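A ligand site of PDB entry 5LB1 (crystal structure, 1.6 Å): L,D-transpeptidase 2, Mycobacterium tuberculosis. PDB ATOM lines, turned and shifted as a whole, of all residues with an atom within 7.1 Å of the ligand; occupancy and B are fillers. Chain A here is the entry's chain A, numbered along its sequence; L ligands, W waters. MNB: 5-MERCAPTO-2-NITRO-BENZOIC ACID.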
ATOM      1  N   LYS A 136       1.820  32.869 -14.648  1.00  0.00           N
ATOM      2  CA  LYS A 136       2.383  33.817 -13.687  1.00  0.00           C
ATOM      3  C   LYS A 136       1.303  34.819 -13.214  1.00  0.00           C
ATOM      4  O   LYS A 136       0.243  34.943 -13.824  1.00  0.00           O
ATOM      5  CB  LYS A 136       3.633  34.553 -14.232  1.00  0.00           C
ATOM      6  CG  LYS A 136       3.478  35.179 -15.590  1.00  0.00           C
ATOM      7  CD  LYS A 136       4.830  35.552 -16.215  1.00  0.00           C
ATOM      8  CE  LYS A 136       4.639  36.231 -17.578  1.00  0.00           C
ATOM      9  NZ  LYS A 136       3.932  35.402 -18.582  1.00  0.00           N
ATOM     10  N   ILE A 156       3.646  24.023 -32.948  1.00  0.00           N
ATOM     11  CA  ILE A 156       4.531  25.177 -32.751  1.00  0.00           C
ATOM     12  C   ILE A 156       3.703  26.305 -32.138  1.00  0.00           C
ATOM     13  O   ILE A 156       2.716  26.760 -32.726  1.00  0.00           O
ATOM     14  CB  ILE A 156       5.194  25.633 -34.077  1.00  0.00           C
ATOM     15  CG1 ILE A 156       6.108  24.523 -34.618  1.00  0.00           C
ATOM     16  CG2 ILE A 156       5.945  26.934 -33.863  1.00  0.00           C
ATOM     17  CD1 ILE A 156       6.721  24.776 -35.996  1.00  0.00           C
ATOM     18  N   MET A 157       4.085  26.746 -30.949  1.00  0.00           N
ATOM     19  CA  MET A 157       3.430  27.851 -30.274  1.00  0.00           C
ATOM     20  C   MET A 157       4.362  29.014 -30.443  1.00  0.00           C
ATOM     21  O   MET A 157       5.508  28.956 -29.977  1.00  0.00           O
ATOM     22  CB  MET A 157       3.262  27.565 -28.797  1.00  0.00           C
ATOM     23  CG  MET A 157       2.581  26.256 -28.526  1.00  0.00           C
ATOM     24  SD  MET A 157       0.869  26.388 -28.944  1.00  0.00           S
ATOM     25  CE  MET A 157       0.212  25.119 -27.866  1.00  0.00           C
ATOM     26  N   ASP A 158       3.914  30.041 -31.118  1.00  0.00           N
ATOM     27  CA  ASP A 158       4.779  31.160 -31.376  1.00  0.00           C
ATOM     28  C   ASP A 158       4.186  32.524 -30.982  1.00  0.00           C
ATOM     29  O   ASP A 158       3.051  32.627 -30.556  1.00  0.00           O
ATOM     30  CB  ASP A 158       5.273  31.093 -32.823  1.00  0.00           C
ATOM     31  CG  ASP A 158       4.226  31.398 -33.826  1.00  0.00           C
ATOM     32  OD1 ASP A 158       3.439  32.381 -33.681  1.00  0.00           O
ATOM     33  OD2 ASP A 158       4.241  30.702 -34.849  1.00  0.00           O
ATOM     34  N   SER A 159       5.010  33.553 -31.160  1.00  0.00           N
ATOM     35  CA  SER A 159       4.707  34.889 -30.691  1.00  0.00           C
ATOM     36  C   SER A 159       3.589  35.547 -31.473  1.00  0.00           C
ATOM     37  O   SER A 159       2.997  36.494 -30.953  1.00  0.00           O
ATOM     38  CB  SER A 159       5.973  35.766 -30.749  1.00  0.00           C
ATOM     39  OG  SER A 159       6.483  35.785 -32.075  1.00  0.00           O
ATOM     40  N   THR A 161       0.722  34.508 -31.897  1.00  0.00           N
ATOM     41  CA  THR A 161      -0.498  34.352 -31.060  1.00  0.00           C
ATOM     42  C   THR A 161      -0.764  35.594 -30.198  1.00  0.00           C
ATOM     43  O   THR A 161      -1.926  35.887 -29.822  1.00  0.00           O
ATOM     44  CB  THR A 161      -0.415  33.099 -30.159  1.00  0.00           C
ATOM     45  OG1 THR A 161      -0.318  31.927 -30.978  1.00  0.00           O
ATOM     46  CG2 THR A 161      -1.675  32.974 -29.252  1.00  0.00           C
ATOM     47  N   TYR A 162       0.293  36.329 -29.866  1.00  0.00           N
ATOM     48  CA  TYR A 162       0.138  37.529 -29.092  1.00  0.00           C
ATOM     49  C   TYR A 162       0.381  38.791 -29.965  1.00  0.00           C
ATOM     50  O   TYR A 162       0.533  39.895 -29.425  1.00  0.00           O
ATOM     51  CB  TYR A 162       1.054  37.480 -27.854  1.00  0.00           C
ATOM     52  CG  TYR A 162       0.775  36.270 -26.984  1.00  0.00           C
ATOM     53  CD1 TYR A 162      -0.368  36.230 -26.180  1.00  0.00           C
ATOM     54  CD2 TYR A 162       1.595  35.137 -27.014  1.00  0.00           C
ATOM     55  CE1 TYR A 162      -0.665  35.108 -25.414  1.00  0.00           C
ATOM     56  CE2 TYR A 162       1.310  34.016 -26.240  1.00  0.00           C
ATOM     57  CZ  TYR A 162       0.176  34.004 -25.441  1.00  0.00           C
ATOM     58  OH  TYR A 162      -0.105  32.887 -24.675  1.00  0.00           O
ATOM     59  N   TYR A 172       9.401  34.769 -31.167  1.00  0.00           N
ATOM     60  CA  TYR A 172       9.854  33.439 -30.775  1.00  0.00           C
ATOM     61  C   TYR A 172       8.933  32.395 -31.368  1.00  0.00           C
ATOM     62  O   TYR A 172       7.794  32.712 -31.736  1.00  0.00           O
ATOM     63  CB  TYR A 172       9.910  33.285 -29.248  1.00  0.00           C
ATOM     64  CG  TYR A 172       8.579  33.437 -28.573  1.00  0.00           C
ATOM     65  CD1 TYR A 172       7.685  32.340 -28.486  1.00  0.00           C
ATOM     66  CD2 TYR A 172       8.193  34.646 -28.005  1.00  0.00           C
ATOM     67  CE1 TYR A 172       6.460  32.468 -27.868  1.00  0.00           C
ATOM     68  CE2 TYR A 172       6.959  34.779 -27.388  1.00  0.00           C
ATOM     69  CZ  TYR A 172       6.095  33.701 -27.325  1.00  0.00           C
ATOM     70  OH  TYR A 172       4.877  33.842 -26.694  1.00  0.00           O
ATOM     71  N   ARG A 173       9.418  31.151 -31.436  1.00  0.00           N
ATOM     72  CA  ARG A 173       8.628  30.010 -31.840  1.00  0.00           C
ATOM     73  C   ARG A 173       9.137  28.826 -31.025  1.00  0.00           C
ATOM     74  O   ARG A 173      10.351  28.600 -30.922  1.00  0.00           O
ATOM     75  CB  ARG A 173       8.762  29.742 -33.339  1.00  0.00           C
ATOM     76  CG  ARG A 173      10.119  30.136 -33.910  1.00  0.00           C
ATOM     77  CD  ARG A 173      10.586  29.091 -34.893  1.00  0.00           C
ATOM     78  NE  ARG A 173      10.409  27.762 -34.313  1.00  0.00           N
ATOM     79  CZ  ARG A 173      10.231  26.637 -35.009  1.00  0.00           C
ATOM     80  NH1 ARG A 173      10.213  26.649 -36.336  1.00  0.00           N
ATOM     81  NH2 ARG A 173      10.065  25.497 -34.356  1.00  0.00           N
ATOM     82  N   THR A 174       8.199  28.106 -30.419  1.00  0.00           N
ATOM     83  CA  THR A 174       8.510  27.027 -29.467  1.00  0.00           C
ATOM     84  C   THR A 174       7.920  25.724 -29.962  1.00  0.00           C
ATOM     85  O   THR A 174       6.682  25.630 -30.181  1.00  0.00           O
ATOM     86  CB  THR A 174       7.871  27.308 -28.087  1.00  0.00           C
ATOM     87  OG1 THR A 174       8.171  28.642 -27.655  1.00  0.00           O
ATOM     88  CG2 THR A 174       8.306  26.301 -27.050  1.00  0.00           C
ATOM     89  N   ASP A 175       8.768  24.717 -30.136  1.00  0.00           N
ATOM     90  CA  ASP A 175       8.315  23.342 -30.360  1.00  0.00           C
ATOM     91  C   ASP A 175       7.726  22.810 -29.060  1.00  0.00           C
ATOM     92  O   ASP A 175       8.396  22.819 -28.023  1.00  0.00           O
ATOM     93  CB  ASP A 175       9.469  22.466 -30.810  1.00  0.00           C
ATOM     94  CG  ASP A 175       9.909  22.783 -32.214  1.00  0.00           C
ATOM     95  OD1 ASP A 175       9.253  22.281 -33.160  1.00  0.00           O
ATOM     96  OD2 ASP A 175      10.920  23.506 -32.379  1.00  0.00           O
ATOM     97  N   VAL A 176       6.469  22.379 -29.132  1.00  0.00           N
ATOM     98  CA  VAL A 176       5.731  21.866 -27.972  1.00  0.00           C
ATOM     99  C   VAL A 176       5.194  20.484 -28.313  1.00  0.00           C
ATOM    100  O   VAL A 176       4.597  20.292 -29.384  1.00  0.00           O
ATOM    101  CB  VAL A 176       4.580  22.805 -27.562  1.00  0.00           C
ATOM    102  CG1 VAL A 176       3.803  22.248 -26.359  1.00  0.00           C
ATOM    103  CG2 VAL A 176       5.095  24.168 -27.168  1.00  0.00           C
ATOM    104  N   GLY A 186      -7.069  29.820 -25.492  1.00  0.00           N
ATOM    105  CA  GLY A 186      -5.703  29.396 -25.719  1.00  0.00           C
ATOM    106  C   GLY A 186      -5.003  28.693 -24.588  1.00  0.00           C
ATOM    107  O   GLY A 186      -3.761  28.655 -24.582  1.00  0.00           O
ATOM    108  N   VAL A 187      -5.767  28.144 -23.631  1.00  0.00           N
ATOM    109  CA  VAL A 187      -5.175  27.343 -22.566  1.00  0.00           C
ATOM    110  C   VAL A 187      -5.021  25.888 -23.035  1.00  0.00           C
ATOM    111  O   VAL A 187      -5.971  25.282 -23.515  1.00  0.00           O
ATOM    112  CB  VAL A 187      -5.993  27.428 -21.259  1.00  0.00           C
ATOM    113  CG1 VAL A 187      -5.359  26.576 -20.147  1.00  0.00           C
ATOM    114  CG2 VAL A 187      -6.110  28.882 -20.795  1.00  0.00           C
ATOM    115  N   PHE A 188      -3.822  25.344 -22.810  1.00  0.00           N
ATOM    116  CA  PHE A 188      -3.483  23.943 -23.115  1.00  0.00           C
ATOM    117  C   PHE A 188      -2.811  23.312 -21.883  1.00  0.00           C
ATOM    118  O   PHE A 188      -2.148  24.009 -21.095  1.00  0.00           O
ATOM    119  CB  PHE A 188      -2.449  23.785 -24.248  1.00  0.00           C
ATOM    120  CG  PHE A 188      -2.938  24.169 -25.628  1.00  0.00           C
ATOM    121  CD1 PHE A 188      -3.145  25.512 -25.946  1.00  0.00           C
ATOM    122  CD2 PHE A 188      -3.182  23.212 -26.601  1.00  0.00           C
ATOM    123  CE1 PHE A 188      -3.570  25.874 -27.211  1.00  0.00           C
ATOM    124  CE2 PHE A 188      -3.619  23.575 -27.860  1.00  0.00           C
ATOM    125  CZ  PHE A 188      -3.824  24.911 -28.156  1.00  0.00           C
ATOM    126  N   HIS A 190       0.274  20.814 -21.554  1.00  0.00           N
ATOM    127  CA  HIS A 190       1.300  20.396 -22.503  1.00  0.00           C
ATOM    128  C   HIS A 190       2.644  20.096 -21.826  1.00  0.00           C
ATOM    129  O   HIS A 190       2.863  20.460 -20.659  1.00  0.00           O
ATOM    130  CB  HIS A 190       1.517  21.488 -23.577  1.00  0.00           C
ATOM    131  CG  HIS A 190       2.093  22.747 -23.038  1.00  0.00           C
ATOM    132  ND1 HIS A 190       3.451  22.952 -22.906  1.00  0.00           N
ATOM    133  CD2 HIS A 190       1.506  23.876 -22.580  1.00  0.00           C
ATOM    134  CE1 HIS A 190       3.672  24.160 -22.396  1.00  0.00           C
ATOM    135  NE2 HIS A 190       2.504  24.737 -22.173  1.00  0.00           N
ATOM    136  N   SER A 191       3.531  19.445 -22.588  1.00  0.00           N
ATOM    137  CA  SER A 191       4.899  19.156 -22.135  1.00  0.00           C
ATOM    138  C   SER A 191       5.703  20.442 -22.001  1.00  0.00           C
ATOM    139  O   SER A 191       5.761  21.232 -22.977  1.00  0.00           O
ATOM    140  CB  SER A 191       5.575  18.212 -23.119  1.00  0.00           C
ATOM    141  OG  SER A 191       6.896  17.933 -22.713  1.00  0.00           O
ATOM    142  N   TRP A 194      11.317  22.663 -19.962  1.00  0.00           N
ATOM    143  CA  TRP A 194      12.089  23.823 -19.455  1.00  0.00           C
ATOM    144  C   TRP A 194      11.695  24.248 -18.032  1.00  0.00           C
ATOM    145  O   TRP A 194      12.469  24.935 -17.352  1.00  0.00           O
ATOM    146  CB  TRP A 194      11.951  25.022 -20.406  1.00  0.00           C
ATOM    147  CG  TRP A 194      10.504  25.483 -20.628  1.00  0.00           C
ATOM    148  CD1 TRP A 194       9.810  26.364 -19.870  1.00  0.00           C
ATOM    149  CD2 TRP A 194       9.626  25.076 -21.687  1.00  0.00           C
ATOM    150  NE1 TRP A 194       8.549  26.548 -20.371  1.00  0.00           N
ATOM    151  CE2 TRP A 194       8.404  25.762 -21.487  1.00  0.00           C
ATOM    152  CE3 TRP A 194       9.761  24.235 -22.787  1.00  0.00           C
ATOM    153  CZ2 TRP A 194       7.306  25.602 -22.342  1.00  0.00           C
ATOM    154  CZ3 TRP A 194       8.664  24.058 -23.639  1.00  0.00           C
ATOM    155  CH2 TRP A 194       7.447  24.745 -23.396  1.00  0.00           C
ATOM    156  N   SER A 205       4.127  30.362 -16.511  1.00  0.00           N
ATOM    157  CA  SER A 205       3.663  30.342 -17.910  1.00  0.00           C
ATOM    158  C   SER A 205       2.868  31.584 -18.280  1.00  0.00           C
ATOM    159  O   SER A 205       2.607  32.444 -17.449  1.00  0.00           O
ATOM    160  CB  SER A 205       2.814  29.110 -18.207  1.00  0.00           C
ATOM    161  OG  SER A 205       1.490  29.307 -17.735  1.00  0.00           O
ATOM    162  N   HIS A 206       2.446  31.606 -19.541  1.00  0.00           N
ATOM    163  CA  HIS A 206       1.583  32.645 -20.065  1.00  0.00           C
ATOM    164  C   HIS A 206       0.107  32.300 -19.817  1.00  0.00           C
ATOM    165  O   HIS A 206      -0.748  33.063 -20.182  1.00  0.00           O
ATOM    166  CB  HIS A 206       1.818  32.878 -21.571  1.00  0.00           C
ATOM    167  CG  HIS A 206       1.596  34.294 -22.012  1.00  0.00           C
ATOM    168  ND1 HIS A 206       2.566  35.027 -22.669  1.00  0.00           N
ATOM    169  CD2 HIS A 206       0.515  35.100 -21.905  1.00  0.00           C
ATOM    170  CE1 HIS A 206       2.085  36.226 -22.945  1.00  0.00           C
ATOM    171  NE2 HIS A 206       0.849  36.304 -22.476  1.00  0.00           N
ATOM    172  N   GLY A 207      -0.185  31.175 -19.165  1.00  0.00           N
ATOM    173  CA  GLY A 207      -1.560  30.762 -18.923  1.00  0.00           C
ATOM    174  C   GLY A 207      -1.745  29.263 -19.061  1.00  0.00           C
ATOM    175  O   GLY A 207      -2.669  28.699 -18.461  1.00  0.00           O
ATOM    176  N   CYS A 208      -0.899  28.602 -19.852  1.00  0.00           N
ATOM    177  CA  CYS A 208      -1.018  27.175 -20.065  1.00  0.00           C
ATOM    178  C   CYS A 208      -0.616  26.406 -18.785  1.00  0.00           C
ATOM    179  O   CYS A 208       0.114  26.920 -17.931  1.00  0.00           O
ATOM    180  CB  CYS A 208      -0.174  26.704 -21.265  1.00  0.00           C
ATOM    181  SG  CYS A 208      -0.936  27.226 -22.790  1.00  0.00           S
ATOM    182  N   LEU A 209      -1.063  25.153 -18.692  1.00  0.00           N
ATOM    183  CA  LEU A 209      -0.708  24.243 -17.582  1.00  0.00           C
ATOM    184  C   LEU A 209       0.530  23.445 -18.043  1.00  0.00           C
ATOM    185  O   LEU A 209       0.398  22.488 -18.810  1.00  0.00           O
ATOM    186  CB  LEU A 209      -1.887  23.283 -17.224  1.00  0.00           C
ATOM    187  CG  LEU A 209      -3.018  23.908 -16.375  1.00  0.00           C
ATOM    188  CD1 LEU A 209      -3.776  24.982 -17.152  1.00  0.00           C
ATOM    189  CD2 LEU A 209      -4.007  22.876 -15.908  1.00  0.00           C
ATOM    190  N   ASN A 210       1.715  23.853 -17.588  1.00  0.00           N
ATOM    191  CA  ASN A 210       2.934  23.119 -17.895  1.00  0.00           C
ATOM    192  C   ASN A 210       3.002  21.853 -17.036  1.00  0.00           C
ATOM    193  O   ASN A 210       2.859  21.953 -15.816  1.00  0.00           O
ATOM    194  CB  ASN A 210       4.158  23.940 -17.521  1.00  0.00           C
ATOM    195  CG  ASN A 210       4.404  25.175 -18.382  1.00  0.00           C
ATOM    196  OD1 ASN A 210       3.602  25.592 -19.257  1.00  0.00           O
ATOM    197  ND2 ASN A 210       5.533  25.762 -18.143  1.00  0.00           N
HETATM  198  C6  MNB L   1       2.015  29.884 -24.406  1.00  0.00           C
HETATM  199  C1  MNB L   1       3.293  29.843 -24.894  1.00  0.00           C
HETATM  200  C2  MNB L   1       3.940  28.544 -25.117  1.00  0.00           C
HETATM  201  C3  MNB L   1       3.255  27.358 -24.818  1.00  0.00           C
HETATM  202  C4  MNB L   1       1.949  27.448 -24.318  1.00  0.00           C
HETATM  203  C5  MNB L   1       1.348  28.700 -24.120  1.00  0.00           C
HETATM  204  S5  MNB L   1      -0.202  28.943 -23.458  1.00  0.00           S
HETATM  205  C10 MNB L   1       4.020  31.103 -25.205  1.00  0.00           C
HETATM  206  O12 MNB L   1       4.898  31.483 -24.393  1.00  0.00           O
HETATM  207  O11 MNB L   1       3.743  31.743 -26.241  1.00  0.00           O
HETATM  208  N7  MNB L   1       5.252  28.529 -25.623  1.00  0.00           N
HETATM  209  O9  MNB L   1       6.008  27.396 -25.433  1.00  0.00           O
HETATM  210  O8  MNB L   1       5.840  29.623 -26.249  1.00  0.00           O
HETATM  211  O   HOH W   1       3.470  27.484 -21.500  1.00  0.00           O
HETATM  212  O   HOH W   2       4.359  30.329 -21.754  1.00  0.00           O
HETATM  213  O   HOH W   3       2.000  30.872 -28.320  1.00  0.00           O
HETATM  214  O   HOH W   4       1.619  29.676 -21.321  1.00  0.00           O
HETATM  215  O   HOH W   5       5.089  34.072 -23.294  1.00  0.00           O
HETATM  216  O   HOH W   6      -2.832  30.402 -22.138  1.00  0.00           O
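The backbone carbonyl oxygen of Tyr 172 sits at hydrogen-bond distance from the backbone NH of Ser 159 (3.0 Å).
The side-chain sulfur of Cys 208 sits at hydrogen-bond distance from the backbone NH of Phe 188.
OD1 of Asn 210 sits at hydrogen-bond distance from NE2 of His 190 (3.2 Å).
N of His 190 is in hydrogen-bond range of O of Leu 209 (3.2 Å).
O of Met 157 is in hydrogen-bond range of N of Thr 174 (2.9 Å).
The backbone carbonyl oxygen (O) of Cys 208 is in hydrogen-bond range of the side-chain hydroxyl (OG) of Ser 205 (2.8 Å).
A sulfur (S5) of the ligand lies close to the backbone carbonyl oxygen (O) of Gly 186.
O of Met 157 touches O8 of the ligand (3.8 Å).
CE2 of Tyr 162 touches O11 of the ligand, 3.3 Å away.
Val 176 touches the ligand.
His 190 touches the ligand.
Trp 194 touches the ligand (CH2 to O9, 3.6 Å).
Hydrophobic or aromatic side chains that line the ligand: Met 157, Tyr 162, Tyr 172, Val 176, His 190 and Trp 194.
Within 4 Å of the ligand: Met 157, Tyr 162, Tyr 172, Thr 174, Val 176, Gly 186, His 190, Trp 194 and Cys 208.
Water W5 lies within hydrogen-bond range of ND1 of His 206, O12 of the ligand and OH of Tyr 172.
Water W3 bridges O11 of the ligand (2.8 Å) and O of Asp 158 (3.0 Å).
Water W2 bridges O12 of the ligand (2.9 Å) and N of His 206 (3.2 Å).
Water W1 bridges the side-chain amide oxygen of Asn 210 (2.9 Å) and a ring nitrogen (NE2) of His 190 (3.0 Å).
Water W6 lies within hydrogen-bond range of O of Gly 186 (3.1 Å), S5 of the ligand (3.3 Å) and N of Cys 208 (3.5 Å).
S5 of the ligand is covalently linked to SG of Cys 208.
The backbone NH of Cys 208 lies close to a sulfur (S5) of the ligand, at 3.7 Å.
An oxygen (O11) of the ligand sits at hydrogen-bond distance from the side-chain hydroxyl (OH) of Tyr 172, 2.4 Å away.
OG1 of Thr 174 sits at hydrogen-bond distance from O8 of the ligand, at 2.9 Å.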
